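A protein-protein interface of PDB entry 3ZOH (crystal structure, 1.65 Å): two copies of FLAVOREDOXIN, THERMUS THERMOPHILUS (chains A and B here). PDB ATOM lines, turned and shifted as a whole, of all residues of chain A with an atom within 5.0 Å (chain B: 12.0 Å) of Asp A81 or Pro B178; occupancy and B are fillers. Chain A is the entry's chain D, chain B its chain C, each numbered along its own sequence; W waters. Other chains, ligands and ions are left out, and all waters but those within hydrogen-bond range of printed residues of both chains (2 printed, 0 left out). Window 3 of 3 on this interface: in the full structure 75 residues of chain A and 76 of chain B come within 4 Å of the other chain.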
ATOM      1  N   GLY A  78       0.372  13.703 -10.167  1.00  0.00           N
ATOM      2  CA  GLY A  78      -0.243  13.279 -11.426  1.00  0.00           C
ATOM      3  C   GLY A  78      -1.588  12.594 -11.248  1.00  0.00           C
ATOM      4  O   GLY A  78      -2.422  12.629 -12.147  1.00  0.00           O
ATOM      5  N   GLN A  79      -1.804  11.970 -10.085  1.00  0.00           N
ATOM      6  CA  GLN A  79      -3.041  11.246  -9.807  1.00  0.00           C
ATOM      7  C   GLN A  79      -4.068  12.086  -9.038  1.00  0.00           C
ATOM      8  O   GLN A  79      -5.024  11.550  -8.488  1.00  0.00           O
ATOM      9  CB  GLN A  79      -2.753   9.921  -9.082  1.00  0.00           C
ATOM     10  CG  GLN A  79      -2.082   8.862  -9.955  1.00  0.00           C
ATOM     11  CD  GLN A  79      -2.026   7.489  -9.298  1.00  0.00           C
ATOM     12  OE1 GLN A  79      -1.292   7.282  -8.327  1.00  0.00           O
ATOM     13  NE2 GLN A  79      -2.781   6.536  -9.845  1.00  0.00           N
ATOM     14  N   LYS A  80      -3.886  13.402  -9.040  1.00  0.00           N
ATOM     15  CA  LYS A  80      -4.845  14.329  -8.422  1.00  0.00           C
ATOM     16  C   LYS A  80      -6.303  14.064  -8.838  1.00  0.00           C
ATOM     17  O   LYS A  80      -7.214  14.117  -8.005  1.00  0.00           O
ATOM     18  CB  LYS A  80      -4.473  15.781  -8.724  1.00  0.00           C
ATOM     19  CG  LYS A  80      -4.438  16.134 -10.204  1.00  0.00           C
ATOM     20  CD  LYS A  80      -4.346  17.632 -10.409  1.00  0.00           C
ATOM     21  CE  LYS A  80      -4.981  18.064 -11.721  1.00  0.00           C
ATOM     22  NZ  LYS A  80      -4.125  17.699 -12.885  1.00  0.00           N
ATOM     23  N   ASP A  81      -6.532  13.782 -10.123  1.00  0.00           N
ATOM     24  CA  ASP A  81      -7.904  13.555 -10.591  1.00  0.00           C
ATOM     25  C   ASP A  81      -8.531  12.293 -10.020  1.00  0.00           C
ATOM     26  O   ASP A  81      -9.669  12.338  -9.551  1.00  0.00           O
ATOM     27  CB  ASP A  81      -8.005  13.589 -12.126  1.00  0.00           C
ATOM     28  CG  ASP A  81      -7.871  14.992 -12.683  1.00  0.00           C
ATOM     29  OD1 ASP A  81      -7.426  15.890 -11.942  1.00  0.00           O
ATOM     30  OD2 ASP A  81      -8.209  15.209 -13.867  1.00  0.00           O
ATOM     31  N   LEU A  82      -7.790  11.182 -10.041  1.00  0.00           N
ATOM     32  CA  LEU A  82      -8.273   9.913  -9.488  1.00  0.00           C
ATOM     33  C   LEU A  82      -8.552  10.014  -7.991  1.00  0.00           C
ATOM     34  O   LEU A  82      -9.582   9.536  -7.524  1.00  0.00           O
ATOM     35  CB  LEU A  82      -7.284   8.765  -9.786  1.00  0.00           C
ATOM     36  CG  LEU A  82      -7.486   7.375  -9.164  1.00  0.00           C
ATOM     37  CD1 LEU A  82      -8.826   6.767  -9.554  1.00  0.00           C
ATOM     38  CD2 LEU A  82      -6.337   6.451  -9.561  1.00  0.00           C
ATOM     39  N   VAL A  83      -7.625  10.620  -7.249  1.00  0.00           N
ATOM     40  CA  VAL A  83      -7.773  10.762  -5.802  1.00  0.00           C
ATOM     41  C   VAL A  83      -8.999  11.611  -5.484  1.00  0.00           C
ATOM     42  O   VAL A  83      -9.797  11.251  -4.614  1.00  0.00           O
ATOM     43  CB  VAL A  83      -6.517  11.351  -5.132  1.00  0.00           C
ATOM     44  CG1 VAL A  83      -6.737  11.493  -3.624  1.00  0.00           C
ATOM     45  CG2 VAL A  83      -5.312  10.463  -5.407  1.00  0.00           C
ATOM     46  N   HIS A  84      -9.172  12.709  -6.214  1.00  0.00           N
ATOM     47  CA  HIS A  84     -10.337  13.571  -6.004  1.00  0.00           C
ATOM     48  C   HIS A  84     -11.652  12.851  -6.308  1.00  0.00           C
ATOM     49  O   HIS A  84     -12.625  12.991  -5.560  1.00  0.00           O
ATOM     50  CB  HIS A  84     -10.229  14.868  -6.807  1.00  0.00           C
ATOM     51  CG  HIS A  84     -11.347  15.825  -6.540  1.00  0.00           C
ATOM     52  ND1 HIS A  84     -11.543  16.414  -5.308  1.00  0.00           N
ATOM     53  CD2 HIS A  84     -12.352  16.265  -7.335  1.00  0.00           C
ATOM     54  CE1 HIS A  84     -12.613  17.190  -5.360  1.00  0.00           C
ATOM     55  NE2 HIS A  84     -13.121  17.117  -6.578  1.00  0.00           N
ATOM     56  N   TRP A  85     -11.659  12.062  -7.388  1.00  0.00           N
ATOM     57  CA  TRP A  85     -12.821  11.243  -7.749  1.00  0.00           C
ATOM     58  C   TRP A  85     -13.186  10.274  -6.624  1.00  0.00           C
ATOM     59  O   TRP A  85     -14.340  10.235  -6.181  1.00  0.00           O
ATOM     60  CB  TRP A  85     -12.575  10.477  -9.061  1.00  0.00           C
ATOM     61  CG  TRP A  85     -13.781   9.714  -9.532  1.00  0.00           C
ATOM     62  CD1 TRP A  85     -14.865  10.225 -10.199  1.00  0.00           C
ATOM     63  CD2 TRP A  85     -14.042   8.315  -9.353  1.00  0.00           C
ATOM     64  NE1 TRP A  85     -15.779   9.227 -10.451  1.00  0.00           N
ATOM     65  CE2 TRP A  85     -15.297   8.044  -9.953  1.00  0.00           C
ATOM     66  CE3 TRP A  85     -13.324   7.257  -8.778  1.00  0.00           C
ATOM     67  CZ2 TRP A  85     -15.864   6.764  -9.961  1.00  0.00           C
ATOM     68  CZ3 TRP A  85     -13.889   5.976  -8.790  1.00  0.00           C
ATOM     69  CH2 TRP A  85     -15.145   5.744  -9.390  1.00  0.00           C
ATOM     70  N   GLY A 166     -11.594  20.584  -2.051  1.00  0.00           N
ATOM     71  CA  GLY A 166     -11.367  20.241  -3.445  1.00  0.00           C
ATOM     72  C   GLY A 166     -10.211  20.936  -4.127  1.00  0.00           C
ATOM     73  O   GLY A 166     -10.118  20.900  -5.356  1.00  0.00           O
ATOM     74  N   TYR A 168      -6.039  21.207  -4.624  1.00  0.00           N
ATOM     75  CA  TYR A 168      -4.818  20.412  -4.513  1.00  0.00           C
ATOM     76  C   TYR A 168      -3.569  21.142  -4.966  1.00  0.00           C
ATOM     77  O   TYR A 168      -3.638  22.123  -5.713  1.00  0.00           O
ATOM     78  CB  TYR A 168      -4.940  19.136  -5.338  1.00  0.00           C
ATOM     79  CG  TYR A 168      -6.076  18.249  -4.924  1.00  0.00           C
ATOM     80  CD1 TYR A 168      -7.378  18.531  -5.332  1.00  0.00           C
ATOM     81  CD2 TYR A 168      -5.852  17.124  -4.135  1.00  0.00           C
ATOM     82  CE1 TYR A 168      -8.436  17.726  -4.960  1.00  0.00           C
ATOM     83  CE2 TYR A 168      -6.903  16.308  -3.757  1.00  0.00           C
ATOM     84  CZ  TYR A 168      -8.185  16.616  -4.172  1.00  0.00           C
ATOM     85  OH  TYR A 168      -9.232  15.825  -3.816  1.00  0.00           O
ATOM     86  N   LYS B 151     -11.714  30.679   1.899  1.00  0.00           N
ATOM     87  CA  LYS B 151     -12.374  29.620   2.662  1.00  0.00           C
ATOM     88  C   LYS B 151     -11.573  29.220   3.897  1.00  0.00           C
ATOM     89  O   LYS B 151     -11.848  28.200   4.531  1.00  0.00           O
ATOM     90  CB  LYS B 151     -12.616  28.411   1.761  1.00  0.00           C
ATOM     91  CG  LYS B 151     -13.134  28.808   0.386  1.00  0.00           C
ATOM     92  CD  LYS B 151     -13.546  27.604  -0.439  1.00  0.00           C
ATOM     93  CE  LYS B 151     -14.341  28.047  -1.658  1.00  0.00           C
ATOM     94  NZ  LYS B 151     -14.736  26.889  -2.503  1.00  0.00           N
ATOM     95  N   ARG B 153      -8.189  28.762   3.963  1.00  0.00           N
ATOM     96  CA  ARG B 153      -7.066  27.898   3.605  1.00  0.00           C
ATOM     97  C   ARG B 153      -5.790  28.711   3.424  1.00  0.00           C
ATOM     98  O   ARG B 153      -5.776  29.680   2.667  1.00  0.00           O
ATOM     99  CB  ARG B 153      -7.399  27.123   2.326  1.00  0.00           C
ATOM    100  CG  ARG B 153      -8.646  26.255   2.460  1.00  0.00           C
ATOM    101  CD  ARG B 153      -9.112  25.675   1.130  1.00  0.00           C
ATOM    102  NE  ARG B 153      -9.379  26.718   0.138  1.00  0.00           N
ATOM    103  CZ  ARG B 153     -10.019  26.517  -1.012  1.00  0.00           C
ATOM    104  NH1 ARG B 153     -10.480  25.311  -1.326  1.00  0.00           N
ATOM    105  NH2 ARG B 153     -10.202  27.530  -1.851  1.00  0.00           N
ATOM    106  N   GLU B 174       1.444  26.740  -7.709  1.00  0.00           N
ATOM    107  CA  GLU B 174       0.423  26.195  -8.601  1.00  0.00           C
ATOM    108  C   GLU B 174      -0.549  25.293  -7.842  1.00  0.00           C
ATOM    109  O   GLU B 174      -0.131  24.414  -7.083  1.00  0.00           O
ATOM    110  CB  GLU B 174       1.055  25.450  -9.787  1.00  0.00           C
ATOM    111  CG  GLU B 174       1.806  24.165  -9.445  1.00  0.00           C
ATOM    112  CD  GLU B 174       1.542  23.051 -10.447  1.00  0.00           C
ATOM    113  OE1 GLU B 174       0.488  23.090 -11.112  1.00  0.00           O
ATOM    114  OE2 GLU B 174       2.382  22.136 -10.573  1.00  0.00           O
ATOM    115  N   THR B 175      -1.842  25.526  -8.027  1.00  0.00           N
ATOM    116  CA  THR B 175      -2.856  24.657  -7.430  1.00  0.00           C
ATOM    117  C   THR B 175      -3.765  24.022  -8.485  1.00  0.00           C
ATOM    118  O   THR B 175      -3.796  24.465  -9.638  1.00  0.00           O
ATOM    119  CB  THR B 175      -3.684  25.373  -6.338  1.00  0.00           C
ATOM    120  OG1 THR B 175      -4.150  26.638  -6.818  1.00  0.00           O
ATOM    121  CG2 THR B 175      -2.855  25.576  -5.072  1.00  0.00           C
ATOM    122  N   PHE B 176      -4.472  22.965  -8.096  1.00  0.00           N
ATOM    123  CA  PHE B 176      -5.451  22.310  -8.962  1.00  0.00           C
ATOM    124  C   PHE B 176      -6.788  22.179  -8.229  1.00  0.00           C
ATOM    125  O   PHE B 176      -6.832  21.741  -7.071  1.00  0.00           O
ATOM    126  CB  PHE B 176      -5.008  20.898  -9.352  1.00  0.00           C
ATOM    127  CG  PHE B 176      -3.539  20.751  -9.652  1.00  0.00           C
ATOM    128  CD1 PHE B 176      -3.022  21.128 -10.893  1.00  0.00           C
ATOM    129  CD2 PHE B 176      -2.679  20.173  -8.715  1.00  0.00           C
ATOM    130  CE1 PHE B 176      -1.672  20.966 -11.174  1.00  0.00           C
ATOM    131  CE2 PHE B 176      -1.325  20.009  -8.992  1.00  0.00           C
ATOM    132  CZ  PHE B 176      -0.824  20.404 -10.224  1.00  0.00           C
ATOM    133  N   ALA B 177      -7.871  22.549  -8.909  1.00  0.00           N
ATOM    134  CA  ALA B 177      -9.224  22.287  -8.423  1.00  0.00           C
ATOM    135  C   ALA B 177      -9.989  21.476  -9.479  1.00  0.00           C
ATOM    136  O   ALA B 177     -10.701  22.050 -10.300  1.00  0.00           O
ATOM    137  CB  ALA B 177      -9.944  23.592  -8.092  1.00  0.00           C
ATOM    138  N   PRO B 178      -9.834  20.134  -9.460  1.00  0.00           N
ATOM    139  CA  PRO B 178     -10.290  19.224 -10.530  1.00  0.00           C
ATOM    140  C   PRO B 178     -11.795  19.241 -10.783  1.00  0.00           C
ATOM    141  O   PRO B 178     -12.239  19.116 -11.928  1.00  0.00           O
ATOM    142  CB  PRO B 178      -9.871  17.835 -10.021  1.00  0.00           C
ATOM    143  CG  PRO B 178      -8.825  18.092  -8.988  1.00  0.00           C
ATOM    144  CD  PRO B 178      -9.225  19.387  -8.344  1.00  0.00           C
ATOM    145  OXT PRO B 178     -12.598  19.369  -9.857  1.00  0.00           O
HETATM  146  O   HOH W   1     -12.397  20.607  -6.952  1.00  0.00           O
HETATM  147  O   HOH W   2     -11.331  15.956 -12.570  1.00  0.00           O
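The side-chain carboxylate of Asp A81 is in salt-bridge range of the side-chain amino group of Lys A80 (3.9 Å).
ND1 of His A84 is in hydrogen-bond range of OH of Tyr A168 (2.8 Å).
Asp A81 touches one residue of chain B.
Pro B178 touches four residues of chain A.
Gly A78 touches none of the printed residues of chain B.
Of chain B, only Phe B176 comes within 4 Å of Lys A80.
No residue of chain B comes within 4 Å of Leu A82.
Val A83 touches none of the printed residues of chain B.
Of chain B, only Pro B178 comes within 4 Å of His A84.
Gly A166 touches three residues of chain B.
Of the printed residues of chain A, Ala B177 touches Gly A166.
Printed residues of chain A within 4 Å of Thr B175: Tyr A168 (3.2 Å).
Printed residues of chain A within 4 Å of Phe B176: Lys A80 (3.3 Å), Gly A166 (3.8 Å) and Tyr A168 (2.6 Å).
Arg B153 touches none of the printed residues of chain A.
The nearest residue of chain A that does not touch Pro B178 is Lys A80 (4.4 Å).
CD of Lys A80 touches CG of Phe B176, at 3.3 Å.
Asp A81 touches Pro B178 (OD1 to CB, 3.7 Å).
His A84 touches Pro B178 (CD2 to CB, 3.98 Å).
Gly A166 touches Phe B176.
Gly A166 touches Ala B177 (O to CA, 3.5 Å).
Gly A166 touches Pro B178.
Thr B175 touches Tyr A168.
Tyr A168 touches Pro B178 (CD1 to CD, 3.6 Å).
O of Phe B176 is in hydrogen-bond range of N of Tyr A168 (2.6 Å).
No position is printed for both chains.
Of the 10 printed residues of chain A, 5 touch a printed residue of chain B.
Hydrophobic or aromatic side chains of chain B that line the printed part of chain A: Phe B176, Ala B177 and Pro B178.
Along chain B the printed residues that touch a printed residue of chain A span positions 175 to 178.
Among the printed residues, 9 pairs touch across the chains.
Among the printed residues, no Asp or Glu carboxylate lies within 4 Å of a Lys or Arg side-chain nitrogen of the other chain.
Water W1 bridges the backbone carbonyl oxygen (O) of Gly A166 (2.8 Å) and the chain-end carboxylate (OXT) of Pro B178 (3.2 Å).
Water W2 lies within hydrogen-bond range of O of Pro B178 (3.3 Å) and OD2 of Asp A81 (3.5 Å).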
